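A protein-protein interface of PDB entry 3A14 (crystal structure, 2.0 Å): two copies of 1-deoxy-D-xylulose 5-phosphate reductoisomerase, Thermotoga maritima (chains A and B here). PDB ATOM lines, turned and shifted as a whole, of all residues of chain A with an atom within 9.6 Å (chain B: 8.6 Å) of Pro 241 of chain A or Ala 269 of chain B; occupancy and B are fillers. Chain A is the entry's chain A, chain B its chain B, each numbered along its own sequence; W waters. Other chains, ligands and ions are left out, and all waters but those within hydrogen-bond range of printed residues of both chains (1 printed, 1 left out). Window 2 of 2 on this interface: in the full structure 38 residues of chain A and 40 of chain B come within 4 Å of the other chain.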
ATOM      1  N   GLU A 153      29.469 -11.974 -22.231  1.00  0.00           N
ATOM      2  CA  GLU A 153      30.528 -11.032 -21.871  1.00  0.00           C
ATOM      3  C   GLU A 153      30.038  -9.990 -20.868  1.00  0.00           C
ATOM      4  O   GLU A 153      28.856  -9.946 -20.595  1.00  0.00           O
ATOM      5  CB  GLU A 153      31.170 -10.388 -23.100  1.00  0.00           C
ATOM      6  CG  GLU A 153      30.262 -10.042 -24.213  1.00  0.00           C
ATOM      7  CD  GLU A 153      31.057  -9.584 -25.428  1.00  0.00           C
ATOM      8  OE1 GLU A 153      31.303 -10.415 -26.335  1.00  0.00           O
ATOM      9  OE2 GLU A 153      31.435  -8.392 -25.457  1.00  0.00           O
ATOM     10  N   PRO A 154      30.952  -9.173 -20.294  1.00  0.00           N
ATOM     11  CA  PRO A 154      30.566  -8.278 -19.193  1.00  0.00           C
ATOM     12  C   PRO A 154      29.554  -7.222 -19.574  1.00  0.00           C
ATOM     13  O   PRO A 154      28.802  -6.778 -18.725  1.00  0.00           O
ATOM     14  CB  PRO A 154      31.890  -7.618 -18.792  1.00  0.00           C
ATOM     15  CG  PRO A 154      32.920  -8.565 -19.252  1.00  0.00           C
ATOM     16  CD  PRO A 154      32.402  -9.100 -20.553  1.00  0.00           C
ATOM     17  N   GLU A 155      29.519  -6.819 -20.837  1.00  0.00           N
ATOM     18  CA  GLU A 155      28.607  -5.770 -21.221  1.00  0.00           C
ATOM     19  C   GLU A 155      27.638  -6.256 -22.303  1.00  0.00           C
ATOM     20  O   GLU A 155      28.044  -6.505 -23.436  1.00  0.00           O
ATOM     21  CB  GLU A 155      29.389  -4.525 -21.660  1.00  0.00           C
ATOM     22  CG  GLU A 155      30.109  -4.654 -23.011  1.00  0.00           C
ATOM     23  CD  GLU A 155      31.494  -5.281 -22.948  1.00  0.00           C
ATOM     24  OE1 GLU A 155      31.596  -6.532 -22.918  1.00  0.00           O
ATOM     25  OE2 GLU A 155      32.488  -4.514 -22.982  1.00  0.00           O
ATOM     26  N   VAL A 156      26.368  -6.421 -21.945  1.00  0.00           N
ATOM     27  CA  VAL A 156      25.364  -6.927 -22.885  1.00  0.00           C
ATOM     28  C   VAL A 156      24.156  -6.018 -22.846  1.00  0.00           C
ATOM     29  O   VAL A 156      23.888  -5.372 -21.819  1.00  0.00           O
ATOM     30  CB  VAL A 156      24.936  -8.410 -22.607  1.00  0.00           C
ATOM     31  CG1 VAL A 156      26.099  -9.360 -22.794  1.00  0.00           C
ATOM     32  CG2 VAL A 156      24.310  -8.573 -21.215  1.00  0.00           C
ATOM     33  N   GLU A 157      23.454  -5.918 -23.971  1.00  0.00           N
ATOM     34  CA  GLU A 157      22.172  -5.237 -24.024  1.00  0.00           C
ATOM     35  C   GLU A 157      21.137  -6.189 -23.457  1.00  0.00           C
ATOM     36  O   GLU A 157      20.392  -5.847 -22.540  1.00  0.00           O
ATOM     37  CB  GLU A 157      21.784  -4.925 -25.469  1.00  0.00           C
ATOM     38  CG  GLU A 157      22.484  -3.737 -26.067  1.00  0.00           C
ATOM     39  CD  GLU A 157      22.041  -2.429 -25.448  1.00  0.00           C
ATOM     40  OE1 GLU A 157      22.926  -1.561 -25.245  1.00  0.00           O
ATOM     41  OE2 GLU A 157      20.820  -2.274 -25.160  1.00  0.00           O
ATOM     42  N   LYS A 158      21.091  -7.390 -24.026  1.00  0.00           N
ATOM     43  CA  LYS A 158      20.078  -8.384 -23.682  1.00  0.00           C
ATOM     44  C   LYS A 158      20.629  -9.795 -23.813  1.00  0.00           C
ATOM     45  O   LYS A 158      21.474 -10.071 -24.668  1.00  0.00           O
ATOM     46  CB  LYS A 158      18.860  -8.254 -24.608  1.00  0.00           C
ATOM     47  CG  LYS A 158      18.079  -6.971 -24.436  1.00  0.00           C
ATOM     48  CD  LYS A 158      16.610  -7.258 -24.264  1.00  0.00           C
ATOM     49  CE  LYS A 158      15.849  -6.014 -23.792  1.00  0.00           C
ATOM     50  NZ  LYS A 158      16.365  -5.538 -22.466  1.00  0.00           N
ATOM     51  N   LYS A 223      17.423  -7.373 -18.315  1.00  0.00           N
ATOM     52  CA  LYS A 223      18.325  -7.695 -19.415  1.00  0.00           C
ATOM     53  C   LYS A 223      18.043  -9.044 -20.044  1.00  0.00           C
ATOM     54  O   LYS A 223      18.713  -9.413 -20.998  1.00  0.00           O
ATOM     55  CB  LYS A 223      19.773  -7.631 -18.951  1.00  0.00           C
ATOM     56  CG  LYS A 223      20.294  -6.227 -18.810  1.00  0.00           C
ATOM     57  CD  LYS A 223      21.810  -6.202 -18.876  1.00  0.00           C
ATOM     58  CE  LYS A 223      22.351  -4.776 -18.807  1.00  0.00           C
ATOM     59  NZ  LYS A 223      21.840  -3.930 -19.920  1.00  0.00           N
ATOM     60  N   VAL A 238      23.207 -13.476 -27.241  1.00  0.00           N
ATOM     61  CA  VAL A 238      23.647 -12.335 -26.466  1.00  0.00           C
ATOM     62  C   VAL A 238      23.642 -11.162 -27.436  1.00  0.00           C
ATOM     63  O   VAL A 238      24.286 -11.212 -28.480  1.00  0.00           O
ATOM     64  CB  VAL A 238      25.024 -12.622 -25.819  1.00  0.00           C
ATOM     65  CG1 VAL A 238      25.681 -11.377 -25.345  1.00  0.00           C
ATOM     66  CG2 VAL A 238      24.827 -13.587 -24.625  1.00  0.00           C
ATOM     67  N   VAL A 239      22.857 -10.147 -27.097  1.00  0.00           N
ATOM     68  CA  VAL A 239      22.711  -8.929 -27.891  1.00  0.00           C
ATOM     69  C   VAL A 239      23.637  -7.920 -27.243  1.00  0.00           C
ATOM     70  O   VAL A 239      23.520  -7.657 -26.054  1.00  0.00           O
ATOM     71  CB  VAL A 239      21.238  -8.413 -27.858  1.00  0.00           C
ATOM     72  CG1 VAL A 239      21.092  -7.057 -28.569  1.00  0.00           C
ATOM     73  CG2 VAL A 239      20.283  -9.455 -28.463  1.00  0.00           C
ATOM     74  N   LEU A 240      24.579  -7.386 -28.019  1.00  0.00           N
ATOM     75  CA  LEU A 240      25.636  -6.539 -27.477  1.00  0.00           C
ATOM     76  C   LEU A 240      25.349  -5.092 -27.805  1.00  0.00           C
ATOM     77  O   LEU A 240      24.581  -4.831 -28.727  1.00  0.00           O
ATOM     78  CB  LEU A 240      27.001  -6.962 -28.042  1.00  0.00           C
ATOM     79  CG  LEU A 240      27.269  -8.401 -27.593  1.00  0.00           C
ATOM     80  CD1 LEU A 240      27.920  -9.239 -28.647  1.00  0.00           C
ATOM     81  CD2 LEU A 240      28.008  -8.454 -26.283  1.00  0.00           C
ATOM     82  N   PRO A 241      25.969  -4.151 -27.064  1.00  0.00           N
ATOM     83  CA  PRO A 241      25.699  -2.705 -27.239  1.00  0.00           C
ATOM     84  C   PRO A 241      25.948  -2.180 -28.654  1.00  0.00           C
ATOM     85  O   PRO A 241      25.303  -1.218 -29.061  1.00  0.00           O
ATOM     86  CB  PRO A 241      26.653  -2.033 -26.230  1.00  0.00           C
ATOM     87  CG  PRO A 241      26.976  -3.076 -25.246  1.00  0.00           C
ATOM     88  CD  PRO A 241      26.958  -4.393 -25.991  1.00  0.00           C
ATOM     89  N   ASP A 242      26.844  -2.844 -29.409  1.00  0.00           N
ATOM     90  CA  ASP A 242      27.319  -2.341 -30.710  1.00  0.00           C
ATOM     91  C   ASP A 242      26.550  -2.768 -31.978  1.00  0.00           C
ATOM     92  O   ASP A 242      26.866  -2.311 -33.067  1.00  0.00           O
ATOM     93  CB  ASP A 242      28.826  -2.649 -30.862  1.00  0.00           C
ATOM     94  CG  ASP A 242      29.136  -4.148 -30.832  1.00  0.00           C
ATOM     95  OD1 ASP A 242      28.199  -4.948 -30.766  1.00  0.00           O
ATOM     96  OD2 ASP A 242      30.322  -4.523 -30.874  1.00  0.00           O
ATOM     97  N   GLY A 243      25.555  -3.636 -31.852  1.00  0.00           N
ATOM     98  CA  GLY A 243      24.858  -4.175 -33.026  1.00  0.00           C
ATOM     99  C   GLY A 243      25.169  -5.646 -33.281  1.00  0.00           C
ATOM    100  O   GLY A 243      24.412  -6.343 -33.951  1.00  0.00           O
ATOM    101  N   ASN A 244      26.277  -6.128 -32.726  1.00  0.00           N
ATOM    102  CA  ASN A 244      26.648  -7.539 -32.865  1.00  0.00           C
ATOM    103  C   ASN A 244      25.708  -8.397 -32.024  1.00  0.00           C
ATOM    104  O   ASN A 244      25.248  -7.960 -30.960  1.00  0.00           O
ATOM    105  CB  ASN A 244      28.114  -7.757 -32.443  1.00  0.00           C
ATOM    106  CG  ASN A 244      29.116  -7.397 -33.548  1.00  0.00           C
ATOM    107  OD1 ASN A 244      30.019  -6.590 -33.345  1.00  0.00           O
ATOM    108  ND2 ASN A 244      28.965  -8.006 -34.703  1.00  0.00           N
ATOM    109  N   VAL A 245      25.415  -9.599 -32.522  1.00  0.00           N
ATOM    110  CA  VAL A 245      24.669 -10.627 -31.784  1.00  0.00           C
ATOM    111  C   VAL A 245      25.436 -11.936 -31.915  1.00  0.00           C
ATOM    112  O   VAL A 245      25.754 -12.376 -33.028  1.00  0.00           O
ATOM    113  CB  VAL A 245      23.190 -10.801 -32.294  1.00  0.00           C
ATOM    114  CG1 VAL A 245      22.438 -11.838 -31.464  1.00  0.00           C
ATOM    115  CG2 VAL A 245      22.459  -9.461 -32.245  1.00  0.00           C
ATOM    116  N   LYS A 246      25.770 -12.525 -30.772  1.00  0.00           N
ATOM    117  CA  LYS A 246      26.398 -13.831 -30.757  1.00  0.00           C
ATOM    118  C   LYS A 246      25.338 -14.862 -30.408  1.00  0.00           C
ATOM    119  O   LYS A 246      24.704 -14.776 -29.336  1.00  0.00           O
ATOM    120  CB  LYS A 246      27.537 -13.870 -29.735  1.00  0.00           C
ATOM    121  CG  LYS A 246      28.663 -12.911 -30.020  1.00  0.00           C
ATOM    122  CD  LYS A 246      29.926 -13.292 -29.220  1.00  0.00           C
ATOM    123  CE  LYS A 246      30.033 -12.530 -28.004  1.00  0.00           C
ATOM    124  NZ  LYS A 246      30.970 -13.251 -27.076  1.00  0.00           N
ATOM    125  N   VAL B  22      32.979   7.347 -36.383  1.00  0.00           N
ATOM    126  CA  VAL B  22      32.965   6.696 -35.074  1.00  0.00           C
ATOM    127  C   VAL B  22      33.545   7.599 -33.999  1.00  0.00           C
ATOM    128  O   VAL B  22      32.974   7.698 -32.920  1.00  0.00           O
ATOM    129  CB  VAL B  22      33.676   5.323 -35.090  1.00  0.00           C
ATOM    130  CG1 VAL B  22      33.965   4.832 -33.668  1.00  0.00           C
ATOM    131  CG2 VAL B  22      32.830   4.318 -35.878  1.00  0.00           C
ATOM    132  N   LYS B  25      31.000  10.046 -32.725  1.00  0.00           N
ATOM    133  CA  LYS B  25      29.966   9.394 -31.905  1.00  0.00           C
ATOM    134  C   LYS B  25      30.442   8.880 -30.538  1.00  0.00           C
ATOM    135  O   LYS B  25      29.611   8.588 -29.669  1.00  0.00           O
ATOM    136  CB  LYS B  25      29.342   8.219 -32.677  1.00  0.00           C
ATOM    137  CG  LYS B  25      27.917   8.458 -33.147  1.00  0.00           C
ATOM    138  CD  LYS B  25      27.356   7.297 -33.998  1.00  0.00           C
ATOM    139  CE  LYS B  25      27.774   7.392 -35.459  1.00  0.00           C
ATOM    140  NZ  LYS B  25      27.394   8.702 -36.082  1.00  0.00           N
ATOM    141  N   VAL B  26      31.755   8.740 -30.349  1.00  0.00           N
ATOM    142  CA  VAL B  26      32.294   8.024 -29.185  1.00  0.00           C
ATOM    143  C   VAL B  26      33.533   8.701 -28.611  1.00  0.00           C
ATOM    144  O   VAL B  26      34.397   9.152 -29.355  1.00  0.00           O
ATOM    145  CB  VAL B  26      32.671   6.558 -29.543  1.00  0.00           C
ATOM    146  CG1 VAL B  26      32.732   5.707 -28.297  1.00  0.00           C
ATOM    147  CG2 VAL B  26      31.689   5.963 -30.533  1.00  0.00           C
ATOM    148  N   ILE B 256      30.598  -0.805 -37.041  1.00  0.00           N
ATOM    149  CA  ILE B 256      30.552  -1.821 -35.969  1.00  0.00           C
ATOM    150  C   ILE B 256      31.949  -2.436 -35.758  1.00  0.00           C
ATOM    151  O   ILE B 256      32.548  -2.238 -34.713  1.00  0.00           O
ATOM    152  CB  ILE B 256      29.436  -2.889 -36.213  1.00  0.00           C
ATOM    153  CG1 ILE B 256      28.035  -2.320 -35.933  1.00  0.00           C
ATOM    154  CG2 ILE B 256      29.566  -4.069 -35.221  1.00  0.00           C
ATOM    155  CD1 ILE B 256      27.500  -1.316 -36.910  1.00  0.00           C
ATOM    156  N   SER B 259      34.605   0.197 -34.711  1.00  0.00           N
ATOM    157  CA  SER B 259      34.468   0.495 -33.264  1.00  0.00           C
ATOM    158  C   SER B 259      35.035  -0.623 -32.395  1.00  0.00           C
ATOM    159  O   SER B 259      35.778  -0.369 -31.451  1.00  0.00           O
ATOM    160  CB  SER B 259      33.005   0.715 -32.916  1.00  0.00           C
ATOM    161  OG  SER B 259      32.529   1.810 -33.685  1.00  0.00           O
ATOM    162  N   PHE B 263      38.122   0.172 -29.887  1.00  0.00           N
ATOM    163  CA  PHE B 263      37.786   0.243 -28.452  1.00  0.00           C
ATOM    164  C   PHE B 263      37.951  -1.055 -27.665  1.00  0.00           C
ATOM    165  O   PHE B 263      37.907  -1.036 -26.433  1.00  0.00           O
ATOM    166  CB  PHE B 263      36.383   0.833 -28.248  1.00  0.00           C
ATOM    167  CG  PHE B 263      36.304   2.301 -28.554  1.00  0.00           C
ATOM    168  CD1 PHE B 263      36.648   3.247 -27.579  1.00  0.00           C
ATOM    169  CD2 PHE B 263      35.922   2.748 -29.819  1.00  0.00           C
ATOM    170  CE1 PHE B 263      36.596   4.627 -27.863  1.00  0.00           C
ATOM    171  CE2 PHE B 263      35.860   4.125 -30.114  1.00  0.00           C
ATOM    172  CZ  PHE B 263      36.198   5.060 -29.130  1.00  0.00           C
ATOM    173  N   ARG B 266      36.341  -2.896 -24.872  1.00  0.00           N
ATOM    174  CA  ARG B 266      35.064  -2.228 -24.653  1.00  0.00           C
ATOM    175  C   ARG B 266      34.156  -2.334 -25.880  1.00  0.00           C
ATOM    176  O   ARG B 266      34.622  -2.237 -27.027  1.00  0.00           O
ATOM    177  CB  ARG B 266      35.333  -0.761 -24.276  1.00  0.00           C
ATOM    178  CG  ARG B 266      34.176   0.221 -24.444  1.00  0.00           C
ATOM    179  CD  ARG B 266      34.647   1.665 -24.181  1.00  0.00           C
ATOM    180  NE  ARG B 266      33.673   2.652 -24.642  1.00  0.00           N
ATOM    181  CZ  ARG B 266      33.882   3.969 -24.691  1.00  0.00           C
ATOM    182  NH1 ARG B 266      35.044   4.492 -24.301  1.00  0.00           N
ATOM    183  NH2 ARG B 266      32.921   4.767 -25.138  1.00  0.00           N
ATOM    184  N   ARG B 267      32.864  -2.536 -25.645  1.00  0.00           N
ATOM    185  CA  ARG B 267      31.871  -2.477 -26.718  1.00  0.00           C
ATOM    186  C   ARG B 267      31.259  -1.114 -26.669  1.00  0.00           C
ATOM    187  O   ARG B 267      30.829  -0.689 -25.607  1.00  0.00           O
ATOM    188  CB  ARG B 267      30.750  -3.495 -26.508  1.00  0.00           C
ATOM    189  CG  ARG B 267      31.199  -4.934 -26.556  1.00  0.00           C
ATOM    190  CD  ARG B 267      30.840  -5.557 -27.855  1.00  0.00           C
ATOM    191  NE  ARG B 267      31.216  -6.964 -27.900  1.00  0.00           N
ATOM    192  CZ  ARG B 267      31.279  -7.659 -29.027  1.00  0.00           C
ATOM    193  NH1 ARG B 267      30.978  -7.055 -30.185  1.00  0.00           N
ATOM    194  NH2 ARG B 267      31.620  -8.943 -28.998  1.00  0.00           N
ATOM    195  N   VAL B 268      31.190  -0.451 -27.819  1.00  0.00           N
ATOM    196  CA  VAL B 268      30.604   0.881 -27.940  1.00  0.00           C
ATOM    197  C   VAL B 268      29.101   0.744 -28.110  1.00  0.00           C
ATOM    198  O   VAL B 268      28.644  -0.183 -28.775  1.00  0.00           O
ATOM    199  CB  VAL B 268      31.177   1.604 -29.175  1.00  0.00           C
ATOM    200  CG1 VAL B 268      30.472   2.908 -29.405  1.00  0.00           C
ATOM    201  CG2 VAL B 268      32.663   1.817 -29.000  1.00  0.00           C
ATOM    202  N   ALA B 269      28.333   1.659 -27.512  1.00  0.00           N
ATOM    203  CA  ALA B 269      26.894   1.661 -27.692  1.00  0.00           C
ATOM    204  C   ALA B 269      26.538   2.342 -28.998  1.00  0.00           C
ATOM    205  O   ALA B 269      26.723   3.549 -29.158  1.00  0.00           O
ATOM    206  CB  ALA B 269      26.177   2.343 -26.504  1.00  0.00           C
ATOM    207  N   LEU B 270      26.047   1.548 -29.940  1.00  0.00           N
ATOM    208  CA  LEU B 270      25.583   2.046 -31.215  1.00  0.00           C
ATOM    209  C   LEU B 270      24.097   1.705 -31.289  1.00  0.00           C
ATOM    210  O   LEU B 270      23.326   2.130 -30.432  1.00  0.00           O
ATOM    211  CB  LEU B 270      26.414   1.449 -32.377  1.00  0.00           C
ATOM    212  CG  LEU B 270      27.937   1.702 -32.375  1.00  0.00           C
ATOM    213  CD1 LEU B 270      28.692   0.793 -33.347  1.00  0.00           C
ATOM    214  CD2 LEU B 270      28.308   3.177 -32.652  1.00  0.00           C
ATOM    215  N   GLU B 271      23.699   0.924 -32.277  1.00  0.00           N
ATOM    216  CA  GLU B 271      22.321   0.463 -32.406  1.00  0.00           C
ATOM    217  C   GLU B 271      22.266  -1.053 -32.257  1.00  0.00           C
ATOM    218  O   GLU B 271      22.727  -1.780 -33.144  1.00  0.00           O
ATOM    219  CB  GLU B 271      21.743   0.878 -33.759  1.00  0.00           C
ATOM    220  CG  GLU B 271      21.772   2.385 -34.021  1.00  0.00           C
ATOM    221  CD  GLU B 271      20.829   3.151 -33.107  1.00  0.00           C
ATOM    222  OE1 GLU B 271      19.685   2.677 -32.911  1.00  0.00           O
ATOM    223  OE2 GLU B 271      21.237   4.218 -32.585  1.00  0.00           O
ATOM    224  N   PRO B 272      21.709  -1.538 -31.134  1.00  0.00           N
ATOM    225  CA  PRO B 272      21.586  -2.969 -30.905  1.00  0.00           C
ATOM    226  C   PRO B 272      20.634  -3.594 -31.901  1.00  0.00           C
ATOM    227  O   PRO B 272      19.618  -2.990 -32.245  1.00  0.00           O
ATOM    228  CB  PRO B 272      21.013  -3.058 -29.486  1.00  0.00           C
ATOM    229  CG  PRO B 272      21.283  -1.726 -28.883  1.00  0.00           C
ATOM    230  CD  PRO B 272      21.163  -0.766 -30.008  1.00  0.00           C
ATOM    231  N   PHE B 273      20.996  -4.783 -32.368  1.00  0.00           N
ATOM    232  CA  PHE B 273      20.229  -5.554 -33.335  1.00  0.00           C
ATOM    233  C   PHE B 273      19.294  -6.448 -32.537  1.00  0.00           C
ATOM    234  O   PHE B 273      19.743  -7.346 -31.833  1.00  0.00           O
ATOM    235  CB  PHE B 273      21.207  -6.401 -34.178  1.00  0.00           C
ATOM    236  CG  PHE B 273      20.572  -7.156 -35.318  1.00  0.00           C
ATOM    237  CD1 PHE B 273      20.576  -6.625 -36.601  1.00  0.00           C
ATOM    238  CD2 PHE B 273      19.993  -8.405 -35.112  1.00  0.00           C
ATOM    239  CE1 PHE B 273      20.000  -7.308 -37.664  1.00  0.00           C
ATOM    240  CE2 PHE B 273      19.411  -9.109 -36.164  1.00  0.00           C
ATOM    241  CZ  PHE B 273      19.420  -8.558 -37.448  1.00  0.00           C
ATOM    242  N   PHE B 274      17.994  -6.209 -32.624  1.00  0.00           N
ATOM    243  CA  PHE B 274      17.053  -7.039 -31.874  1.00  0.00           C
ATOM    244  C   PHE B 274      16.442  -8.151 -32.735  1.00  0.00           C
ATOM    245  O   PHE B 274      16.129  -7.950 -33.917  1.00  0.00           O
ATOM    246  CB  PHE B 274      16.006  -6.186 -31.133  1.00  0.00           C
ATOM    247  CG  PHE B 274      16.588  -5.366 -29.997  1.00  0.00           C
ATOM    248  CD1 PHE B 274      16.901  -5.965 -28.770  1.00  0.00           C
ATOM    249  CD2 PHE B 274      16.829  -3.998 -30.155  1.00  0.00           C
ATOM    250  CE1 PHE B 274      17.445  -5.210 -27.715  1.00  0.00           C
ATOM    251  CE2 PHE B 274      17.374  -3.238 -29.105  1.00  0.00           C
ATOM    252  CZ  PHE B 274      17.680  -3.849 -27.884  1.00  0.00           C
HETATM  253  O   HOH W   1      24.796  -0.809 -34.512  1.00  0.00           O
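No position is printed for both chains.
Of the 20 pairs that touch across the chains among the printed residues, none has its exchanged pair printed and touching as well.
The side-chain carboxylate (OE2) of Glu 153 of chain A is in salt-bridge range of the guanidinium group (NE) of Arg 267 of chain B, at 2.8 Å.
OE2 of Glu 155 of chain A lies within hydrogen-bond range of N of Arg 267 of chain B, at 3.3 Å.
O of Pro 241 of chain A sits at hydrogen-bond distance from N of Leu 270 of chain B, 3.0 Å away.
OD2 of Asp 242 of chain A is in salt-bridge range of NH1 of Arg 267 of chain B.
The backbone NH (N) of Asp 242 of chain A lies close to the backbone carbonyl oxygen (O) of Val 268 of chain B (3.3 Å).
OD1 of Asn 244 of chain A sits at hydrogen-bond distance from NH1 of Arg 267 of chain B, 3.3 Å away.
Water W1 lies within hydrogen-bond range of the backbone carbonyl oxygen of Glu 271 of chain B (2.7 Å) and the backbone carbonyl oxygen of Asp 242 of chain A (2.9 Å).
OE2 of Glu 155 of chain A touches CA of Arg 266 of chain B (3.8 Å).
Lys 158 of chain A touches Phe 274 of chain B.
CG1 of Val 239 of chain A touches O of Phe 273 of chain B, at 3.5 Å.
CD1 of Leu 240 of chain A touches NH2 of Arg 267 of chain B (3.7 Å).
C of Pro 241 of chain A touches O of Val 268 of chain B (3.4 Å).
Pro 241 of chain A touches Ala 269 of chain B.
CD1 of Leu 270 of chain B touches O of Asp 242 of chain A, at 3.6 Å.
CA of Gly 243 of chain A touches O of Glu 271 of chain B, 3.2 Å away.
Gly 243 of chain A touches Phe 273 of chain B (O to CB, 3.2 Å).
Asn 244 of chain A touches Ile 256 of chain B (OD1 to CG2, 3.2 Å).
Pro 154 of chain A touches none of the printed residues of chain B.
Of the printed residues of chain B, Val 239 of chain A touches Phe 273 (3.5 Å).
Of chain B, only Arg 267 (3.9 Å), Val 268 (3.4 Å), Ala 269 (3.6 Å) and Leu 270 (3.0 Å) come within 4 Å of Pro 241 of chain A.
Printed residues of chain B within 4 Å of Asn 244 of chain A: Ile 256 and Arg 267.
Lys 246 of chain A touches none of the printed residues of chain B.
Of the printed residues of chain A, Arg 266 of chain B touches Glu 155 (3.8 Å).
Of chain A, only Pro 241 (3.4 Å) and Asp 242 (3.2 Å) come within 4 Å of Val 268 of chain B.
Of chain A, only Pro 241 comes within 4 Å of Ala 269 of chain B.
Leu 270 of chain B touches two residues of chain A.
Of the printed residues of chain A, Phe 274 of chain B touches Lys 158 (3.8 Å).
The nearest residue of chain A that does not touch Ala 269 of chain B is Asp 242 of chain A (4.8 Å).
The nearest printed residue of chain B that does not touch Lys 158 of chain A is Pro 272 of chain B (7.0 Å).
Of the 15 printed residues of chain B, 10 touch a printed residue of chain A.
Printed residues of chain B that touch a printed residue of chain A: Ile 256, Arg 266, Arg 267, Val 268, Ala 269, Leu 270, Glu 271, Pro 272, Phe 273 and Phe 274.
Among the printed residues, 20 pairs touch across the chains.
The side-chain carboxylate (OE1) of Glu 153 of chain A lies within salt-bridge range of the side-chain amino group (NZ) of Lys 246 of chain A (3.0 Å).
N of Glu 157 of chain A lies within hydrogen-bond range of O of Val 239 of chain A, at 2.7 Å.
N of Val 239 of chain A sits at hydrogen-bond distance from O of Lys 158 of chain A (2.8 Å).
The side-chain carboxylate of Asp 242 of chain A sits at hydrogen-bond distance from the backbone NH of Asn 244 of chain A.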
